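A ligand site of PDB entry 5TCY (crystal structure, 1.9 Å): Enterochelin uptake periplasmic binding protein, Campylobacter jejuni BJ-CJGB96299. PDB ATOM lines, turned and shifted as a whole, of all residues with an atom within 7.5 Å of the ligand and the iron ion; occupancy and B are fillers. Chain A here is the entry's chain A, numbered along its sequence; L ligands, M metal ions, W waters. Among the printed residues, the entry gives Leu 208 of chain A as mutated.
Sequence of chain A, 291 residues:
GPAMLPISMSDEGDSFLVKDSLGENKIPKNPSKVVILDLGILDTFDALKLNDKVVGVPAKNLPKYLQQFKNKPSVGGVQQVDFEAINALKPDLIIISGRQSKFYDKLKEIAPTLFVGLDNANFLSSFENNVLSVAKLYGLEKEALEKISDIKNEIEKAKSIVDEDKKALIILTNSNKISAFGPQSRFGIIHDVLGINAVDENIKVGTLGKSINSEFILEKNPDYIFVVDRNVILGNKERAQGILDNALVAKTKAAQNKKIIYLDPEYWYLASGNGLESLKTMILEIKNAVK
Merely in contact with the ligand: Val 78 and Leu 234. Hydrophobic or aromatic side chains within 4 Å of the ligand: Val 78, Leu 234 and Tyr 269. Within 4 Å of the ligand: Val 78, Gln 79, Arg 99, Lys 102, Arg 186, Arg 230, Leu 234 and Tyr 269. The nearest printed residue that does not touch the ligand is Ile 233 (4.1 Å).
The side-chain amino group (NZ) of Lys 102 sits at hydrogen-bond distance from an oxygen (O2) of the ligand (2.8 Å). NH2 of Arg 230 lies close to O5 of the ligand, 2.8 Å away. An oxygen (O6) of the ligand lies close to the guanidinium group (NE) of Arg 99, at 2.7 Å. An oxygen (O3) of the ligand lies close to the side-chain amide oxygen (OE1) of Gln 79, at 3.1 Å. The guanidinium group (NH2) of Arg 186 lies close to an oxygen (O4) of the ligand (2.8 Å).
Residues that only touch the iron ion: Arg 230 (3.9 Å). Two residues have an atom within 4 Å of the iron ion: Arg 230 and Tyr 269. Along chain A the residues within 4 Å of the iron ion span positions 230 to 269.
NH1 of Arg 99 is in hydrogen-bond range of O of Leu 270, at 3.1 Å. The guanidinium group (NH2) of Arg 99 lies within hydrogen-bond range of the backbone carbonyl oxygen (O) of Tyr 269, at 2.8 Å. OH of Tyr 269 lies close to NE of Arg 230, 2.7 Å away. NE2 of Gln 100 lies within hydrogen-bond range of O of Val 78. NE2 of Gln 79 sits close to NZ of Lys 102 (3.2 Å). The backbone carbonyl oxygen (O) of Tyr 269 lies within hydrogen-bond range of the guanidinium group (NH2) of Arg 186 (3.3 Å). The backbone carbonyl oxygen (O) of Arg 99 lies within hydrogen-bond range of the side-chain amino group (NZ) of Lys 102, 2.9 Å away. ND2 of Asn 61 lies close to N of Val 78 (3.0 Å).
OH of Tyr 269 binds the iron ion (1.9 Å). An oxygen (O6) of the ligand binds the iron ion (2.1 Å). O4 of the ligand binds the iron ion (2.1 Å). O3 of the ligand binds the iron ion (2.1 Å). Water W1 is bound to the iron ion, at 2.1 Å. O5 of the ligand is bound to the iron ion (2.1 Å).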
ATOM      1  N   ASN A  61      -7.294 -21.190 -30.479  1.00  0.00           N
ATOM      2  CA  ASN A  61      -7.317 -20.634 -29.103  1.00  0.00           C
ATOM      3  C   ASN A  61      -8.440 -19.655 -28.896  1.00  0.00           C
ATOM      4  O   ASN A  61      -8.391 -18.854 -27.936  1.00  0.00           O
ATOM      5  CB  ASN A  61      -5.953 -20.015 -28.779  1.00  0.00           C
ATOM      6  CG  ASN A  61      -4.876 -21.032 -28.743  1.00  0.00           C
ATOM      7  OD1 ASN A  61      -4.813 -21.884 -27.809  1.00  0.00           O
ATOM      8  ND2 ASN A  61      -4.054 -21.017 -29.745  1.00  0.00           N
ATOM      9  N   GLY A  77      -3.318 -21.129 -34.290  1.00  0.00           N
ATOM     10  CA  GLY A  77      -3.374 -20.749 -32.881  1.00  0.00           C
ATOM     11  C   GLY A  77      -2.415 -19.612 -32.588  1.00  0.00           C
ATOM     12  O   GLY A  77      -1.624 -19.239 -33.428  1.00  0.00           O
ATOM     13  N   VAL A  78      -2.520 -19.043 -31.372  1.00  0.00           N
ATOM     14  CA  VAL A  78      -1.602 -17.981 -30.917  1.00  0.00           C
ATOM     15  C   VAL A  78      -0.115 -18.358 -30.934  1.00  0.00           C
ATOM     16  O   VAL A  78       0.729 -17.472 -31.055  1.00  0.00           O
ATOM     17  CB  VAL A  78      -2.015 -17.400 -29.541  1.00  0.00           C
ATOM     18  CG1 VAL A  78      -3.388 -16.710 -29.681  1.00  0.00           C
ATOM     19  CG2 VAL A  78      -2.015 -18.438 -28.439  1.00  0.00           C
ATOM     20  N   GLN A  79       0.175 -19.654 -30.845  1.00  0.00           N
ATOM     21  CA  GLN A  79       1.548 -20.175 -30.873  1.00  0.00           C
ATOM     22  C   GLN A  79       1.861 -20.901 -32.247  1.00  0.00           C
ATOM     23  O   GLN A  79       2.972 -20.747 -32.812  1.00  0.00           O
ATOM     24  CB  GLN A  79       1.657 -21.087 -29.659  1.00  0.00           C
ATOM     25  CG  GLN A  79       2.881 -21.031 -28.740  1.00  0.00           C
ATOM     26  CD  GLN A  79       3.299 -19.685 -28.168  1.00  0.00           C
ATOM     27  OE1 GLN A  79       2.964 -19.293 -27.012  1.00  0.00           O
ATOM     28  NE2 GLN A  79       4.130 -19.015 -28.946  1.00  0.00           N
ATOM     29  N   GLN A  80       0.863 -21.612 -32.795  1.00  0.00           N
ATOM     30  CA  GLN A  80       0.998 -22.437 -33.999  1.00  0.00           C
ATOM     31  C   GLN A  80       0.343 -21.632 -35.155  1.00  0.00           C
ATOM     32  O   GLN A  80      -0.832 -21.796 -35.499  1.00  0.00           O
ATOM     33  CB  GLN A  80       0.380 -23.829 -33.771  1.00  0.00           C
ATOM     34  CG  GLN A  80      -0.090 -24.631 -35.016  1.00  0.00           C
ATOM     35  CD  GLN A  80       0.912 -24.702 -36.200  1.00  0.00           C
ATOM     36  OE1 GLN A  80       0.515 -24.526 -37.376  1.00  0.00           O
ATOM     37  NE2 GLN A  80       2.201 -24.978 -35.888  1.00  0.00           N
ATOM     38  N   SER A  97       0.869  -9.737 -31.380  1.00  0.00           N
ATOM     39  CA  SER A  97       1.527  -9.309 -30.125  1.00  0.00           C
ATOM     40  C   SER A  97       2.705 -10.221 -29.813  1.00  0.00           C
ATOM     41  O   SER A  97       3.280 -10.801 -30.738  1.00  0.00           O
ATOM     42  CB  SER A  97       0.507  -9.221 -29.042  1.00  0.00           C
ATOM     43  OG  SER A  97      -0.114 -10.485 -28.966  1.00  0.00           O
ATOM     44  N   GLY A  98       3.118 -10.279 -28.543  1.00  0.00           N
ATOM     45  CA  GLY A  98       4.454 -10.766 -28.232  1.00  0.00           C
ATOM     46  C   GLY A  98       4.649 -12.243 -28.548  1.00  0.00           C
ATOM     47  O   GLY A  98       5.778 -12.627 -28.851  1.00  0.00           O
ATOM     48  N   ARG A  99       3.568 -13.053 -28.543  1.00  0.00           N
ATOM     49  CA  ARG A  99       3.691 -14.470 -28.923  1.00  0.00           C
ATOM     50  C   ARG A  99       4.185 -14.684 -30.303  1.00  0.00           C
ATOM     51  O   ARG A  99       4.779 -15.698 -30.552  1.00  0.00           O
ATOM     52  CB  ARG A  99       2.404 -15.265 -28.734  1.00  0.00           C
ATOM     53  CG  ARG A  99       2.097 -15.605 -27.311  1.00  0.00           C
ATOM     54  CD  ARG A  99       0.853 -16.450 -27.217  1.00  0.00           C
ATOM     55  NE  ARG A  99       0.508 -16.821 -25.820  1.00  0.00           N
ATOM     56  CZ  ARG A  99      -0.236 -16.099 -24.961  1.00  0.00           C
ATOM     57  NH1 ARG A  99      -0.774 -14.956 -25.307  1.00  0.00           N
ATOM     58  NH2 ARG A  99      -0.473 -16.550 -23.735  1.00  0.00           N
ATOM     59  N   GLN A 100       3.916 -13.756 -31.222  1.00  0.00           N
ATOM     60  CA  GLN A 100       4.273 -13.904 -32.610  1.00  0.00           C
ATOM     61  C   GLN A 100       5.394 -12.996 -33.072  1.00  0.00           C
ATOM     62  O   GLN A 100       5.774 -13.059 -34.217  1.00  0.00           O
ATOM     63  CB  GLN A 100       3.069 -13.680 -33.485  1.00  0.00           C
ATOM     64  CG  GLN A 100       1.882 -14.576 -33.064  1.00  0.00           C
ATOM     65  CD  GLN A 100       0.904 -13.886 -32.159  1.00  0.00           C
ATOM     66  OE1 GLN A 100       0.764 -12.667 -32.201  1.00  0.00           O
ATOM     67  NE2 GLN A 100       0.210 -14.670 -31.317  1.00  0.00           N
ATOM     68  N   SER A 101       6.017 -12.230 -32.174  1.00  0.00           N
ATOM     69  CA  SER A 101       7.185 -11.454 -32.626  1.00  0.00           C
ATOM     70  C   SER A 101       8.310 -12.343 -33.230  1.00  0.00           C
ATOM     71  O   SER A 101       8.996 -11.925 -34.173  1.00  0.00           O
ATOM     72  CB  SER A 101       7.694 -10.465 -31.550  1.00  0.00           C
ATOM     73  OG  SER A 101       7.713 -11.045 -30.297  1.00  0.00           O
ATOM     74  N   LYS A 102       8.492 -13.545 -32.702  1.00  0.00           N
ATOM     75  CA  LYS A 102       9.455 -14.488 -33.312  1.00  0.00           C
ATOM     76  C   LYS A 102       9.152 -14.817 -34.786  1.00  0.00           C
ATOM     77  O   LYS A 102      10.020 -15.353 -35.444  1.00  0.00           O
ATOM     78  CB  LYS A 102       9.598 -15.755 -32.486  1.00  0.00           C
ATOM     79  CG  LYS A 102       8.377 -16.657 -32.449  1.00  0.00           C
ATOM     80  CD  LYS A 102       8.615 -17.897 -31.566  1.00  0.00           C
ATOM     81  CE  LYS A 102       8.323 -17.618 -30.087  1.00  0.00           C
ATOM     82  NZ  LYS A 102       6.865 -17.499 -29.754  1.00  0.00           N
ATOM     83  N   LEU A 172       0.855 -18.785 -10.953  1.00  0.00           N
ATOM     84  CA  LEU A 172       0.488 -19.577 -12.114  1.00  0.00           C
ATOM     85  C   LEU A 172       0.766 -21.078 -11.841  1.00  0.00           C
ATOM     86  O   LEU A 172       1.782 -21.456 -11.254  1.00  0.00           O
ATOM     87  CB  LEU A 172       1.274 -19.094 -13.310  1.00  0.00           C
ATOM     88  CG  LEU A 172       0.891 -19.763 -14.626  1.00  0.00           C
ATOM     89  CD1 LEU A 172       0.685 -18.750 -15.724  1.00  0.00           C
ATOM     90  CD2 LEU A 172       1.923 -20.800 -15.013  1.00  0.00           C
ATOM     91  N   ARG A 186       3.670 -10.208 -16.458  1.00  0.00           N
ATOM     92  CA  ARG A 186       2.522 -10.436 -17.361  1.00  0.00           C
ATOM     93  C   ARG A 186       1.162 -10.341 -16.644  1.00  0.00           C
ATOM     94  O   ARG A 186       0.182 -10.221 -17.328  1.00  0.00           O
ATOM     95  CB  ARG A 186       2.632 -11.796 -18.075  1.00  0.00           C
ATOM     96  CG  ARG A 186       2.305 -12.950 -17.205  1.00  0.00           C
ATOM     97  CD  ARG A 186       2.626 -14.253 -17.889  1.00  0.00           C
ATOM     98  NE  ARG A 186       1.766 -14.427 -19.053  1.00  0.00           N
ATOM     99  CZ  ARG A 186       2.022 -15.307 -20.016  1.00  0.00           C
ATOM    100  NH1 ARG A 186       3.087 -16.115 -19.957  1.00  0.00           N
ATOM    101  NH2 ARG A 186       1.182 -15.399 -21.036  1.00  0.00           N
ATOM    102  N   THR A 207       7.397 -12.844 -18.334  1.00  0.00           N
ATOM    103  CA  THR A 207       6.495 -13.824 -18.831  1.00  0.00           C
ATOM    104  C   THR A 207       6.704 -15.127 -18.127  1.00  0.00           C
ATOM    105  O   THR A 207       5.801 -15.907 -18.104  1.00  0.00           O
ATOM    106  CB  THR A 207       6.670 -13.975 -20.345  1.00  0.00           C
ATOM    107  OG1 THR A 207       7.954 -14.452 -20.596  1.00  0.00           O
ATOM    108  CG2 THR A 207       6.493 -12.629 -21.019  1.00  0.00           C
ATOM    109  N   LEU A 208       7.875 -15.363 -17.540  1.00  0.00           N
ATOM    110  CA  LEU A 208       8.200 -16.644 -16.846  1.00  0.00           C
ATOM    111  C   LEU A 208       8.279 -16.366 -15.346  1.00  0.00           C
ATOM    112  O   LEU A 208       8.880 -15.378 -14.931  1.00  0.00           O
ATOM    113  CB  LEU A 208       9.506 -17.261 -17.395  1.00  0.00           C
ATOM    114  CG  LEU A 208       9.330 -18.627 -18.120  1.00  0.00           C
ATOM    115  CD1 LEU A 208       8.318 -18.567 -19.255  1.00  0.00           C
ATOM    116  CD2 LEU A 208      10.673 -19.140 -18.624  1.00  0.00           C
ATOM    117  N   ARG A 230      -2.734 -22.327 -16.147  1.00  0.00           N
ATOM    118  CA  ARG A 230      -2.219 -22.637 -17.491  1.00  0.00           C
ATOM    119  C   ARG A 230      -2.630 -24.050 -17.971  1.00  0.00           C
ATOM    120  O   ARG A 230      -2.708 -24.297 -19.165  1.00  0.00           O
ATOM    121  CB  ARG A 230      -0.710 -22.486 -17.523  1.00  0.00           C
ATOM    122  CG  ARG A 230      -0.142 -22.451 -18.925  1.00  0.00           C
ATOM    123  CD  ARG A 230       1.327 -22.215 -18.945  1.00  0.00           C
ATOM    124  NE  ARG A 230       1.799 -22.153 -20.338  1.00  0.00           N
ATOM    125  CZ  ARG A 230       2.531 -23.082 -20.928  1.00  0.00           C
ATOM    126  NH1 ARG A 230       2.925 -24.176 -20.272  1.00  0.00           N
ATOM    127  NH2 ARG A 230       2.902 -22.935 -22.191  1.00  0.00           N
ATOM    128  N   ILE A 233      -5.655 -23.876 -20.345  1.00  0.00           N
ATOM    129  CA  ILE A 233      -5.333 -23.468 -21.695  1.00  0.00           C
ATOM    130  C   ILE A 233      -4.631 -24.595 -22.478  1.00  0.00           C
ATOM    131  O   ILE A 233      -4.987 -24.830 -23.598  1.00  0.00           O
ATOM    132  CB  ILE A 233      -4.453 -22.186 -21.679  1.00  0.00           C
ATOM    133  CG1 ILE A 233      -5.216 -21.051 -20.960  1.00  0.00           C
ATOM    134  CG2 ILE A 233      -4.022 -21.757 -23.082  1.00  0.00           C
ATOM    135  CD1 ILE A 233      -6.616 -20.754 -21.582  1.00  0.00           C
ATOM    136  N   LEU A 234      -3.645 -25.273 -21.877  1.00  0.00           N
ATOM    137  CA  LEU A 234      -2.883 -26.330 -22.585  1.00  0.00           C
ATOM    138  C   LEU A 234      -3.597 -27.687 -22.606  1.00  0.00           C
ATOM    139  O   LEU A 234      -3.109 -28.613 -23.244  1.00  0.00           O
ATOM    140  CB  LEU A 234      -1.483 -26.510 -21.989  1.00  0.00           C
ATOM    141  CG  LEU A 234      -0.408 -25.615 -22.589  1.00  0.00           C
ATOM    142  CD1 LEU A 234      -0.765 -24.144 -22.411  1.00  0.00           C
ATOM    143  CD2 LEU A 234       0.909 -25.923 -21.909  1.00  0.00           C
ATOM    144  N   TYR A 269      -4.233 -15.460 -18.996  1.00  0.00           N
ATOM    145  CA  TYR A 269      -3.105 -16.125 -19.602  1.00  0.00           C
ATOM    146  C   TYR A 269      -3.032 -15.844 -21.133  1.00  0.00           C
ATOM    147  O   TYR A 269      -2.041 -15.397 -21.675  1.00  0.00           O
ATOM    148  CB  TYR A 269      -3.146 -17.641 -19.312  1.00  0.00           C
ATOM    149  CG  TYR A 269      -1.854 -18.238 -19.787  1.00  0.00           C
ATOM    150  CD1 TYR A 269      -0.629 -17.986 -19.101  1.00  0.00           C
ATOM    151  CD2 TYR A 269      -1.799 -18.911 -20.984  1.00  0.00           C
ATOM    152  CE1 TYR A 269       0.569 -18.453 -19.611  1.00  0.00           C
ATOM    153  CE2 TYR A 269      -0.598 -19.373 -21.481  1.00  0.00           C
ATOM    154  CZ  TYR A 269       0.591 -19.189 -20.791  1.00  0.00           C
ATOM    155  OH  TYR A 269       1.777 -19.675 -21.407  1.00  0.00           O
ATOM    156  N   LEU A 270      -4.104 -16.112 -21.833  1.00  0.00           N
ATOM    157  CA  LEU A 270      -4.209 -15.773 -23.256  1.00  0.00           C
ATOM    158  C   LEU A 270      -4.073 -14.300 -23.519  1.00  0.00           C
ATOM    159  O   LEU A 270      -3.656 -13.942 -24.583  1.00  0.00           O
ATOM    160  CB  LEU A 270      -5.548 -16.255 -23.783  1.00  0.00           C
ATOM    161  CG  LEU A 270      -5.710 -17.755 -23.946  1.00  0.00           C
ATOM    162  CD1 LEU A 270      -7.002 -18.048 -24.684  1.00  0.00           C
ATOM    163  CD2 LEU A 270      -4.585 -18.370 -24.716  1.00  0.00           C
ATOM    164  N   ALA A 271      -4.409 -13.469 -22.525  1.00  0.00           N
ATOM    165  CA  ALA A 271      -3.837 -12.092 -22.348  1.00  0.00           C
ATOM    166  C   ALA A 271      -4.615 -11.178 -23.298  1.00  0.00           C
ATOM    167  O   ALA A 271      -4.097 -10.675 -24.286  1.00  0.00           O
ATOM    168  CB  ALA A 271      -2.328 -12.039 -22.639  1.00  0.00           C
HETATM  169  C1  LIG L   1      -0.816 -20.074 -25.359  1.00  0.00           C
HETATM  170  C2  LIG L   1       0.439 -20.003 -24.803  1.00  0.00           C
HETATM  171  C3  LIG L   1       1.297 -21.089 -24.814  1.00  0.00           C
HETATM  172  C4  LIG L   1       0.922 -22.254 -25.438  1.00  0.00           C
HETATM  173  C5  LIG L   1      -0.358 -22.315 -26.045  1.00  0.00           C
HETATM  174  C6  LIG L   1      -1.213 -21.236 -25.994  1.00  0.00           C
HETATM  175  C7  LIG L   1       1.903 -23.423 -25.578  1.00  0.00           C
HETATM  176  N1  LIG L   1       3.204 -23.117 -25.366  1.00  0.00           N
HETATM  177  O1  LIG L   1       1.493 -24.518 -25.946  1.00  0.00           O
HETATM  178  C8  LIG L   1       4.344 -24.013 -25.376  1.00  0.00           C
HETATM  179  C9  LIG L   1       5.626 -23.464 -25.996  1.00  0.00           C
HETATM  180  C10 LIG L   1       6.217 -22.167 -25.439  1.00  0.00           C
HETATM  181  N2  LIG L   1       6.213 -18.882 -25.720  1.00  0.00           N
HETATM  182  C11 LIG L   1       6.192 -17.619 -26.044  1.00  0.00           C
HETATM  183  C12 LIG L   1       5.343 -16.665 -25.198  1.00  0.00           C
HETATM  184  O2  LIG L   1       6.868 -17.176 -26.977  1.00  0.00           O
HETATM  185  C13 LIG L   1       4.412 -17.204 -24.345  1.00  0.00           C
HETATM  186  C14 LIG L   1       3.638 -16.411 -23.511  1.00  0.00           C
HETATM  187  C15 LIG L   1       3.767 -15.031 -23.552  1.00  0.00           C
HETATM  188  C16 LIG L   1       4.707 -14.464 -24.425  1.00  0.00           C
HETATM  189  C17 LIG L   1       5.490 -15.261 -25.261  1.00  0.00           C
HETATM  190  O3  LIG L   1       4.221 -18.561 -24.264  1.00  0.00           O
HETATM  191  O4  LIG L   1       2.789 -17.072 -22.654  1.00  0.00           O
HETATM  192  C18 LIG L   1       6.612 -21.219 -26.558  1.00  0.00           C
HETATM  193  O5  LIG L   1       2.509 -20.962 -24.181  1.00  0.00           O
HETATM  194  C19 LIG L   1       7.173 -19.856 -26.257  1.00  0.00           C
HETATM  195  O6  LIG L   1       0.875 -18.913 -24.154  1.00  0.00           O
HETATM  196 FE    FE M   1       2.591 -19.163 -23.024  1.00  0.00          FE
HETATM  197  O   HOH W   1       4.330 -19.996 -22.098  1.00  0.00           O
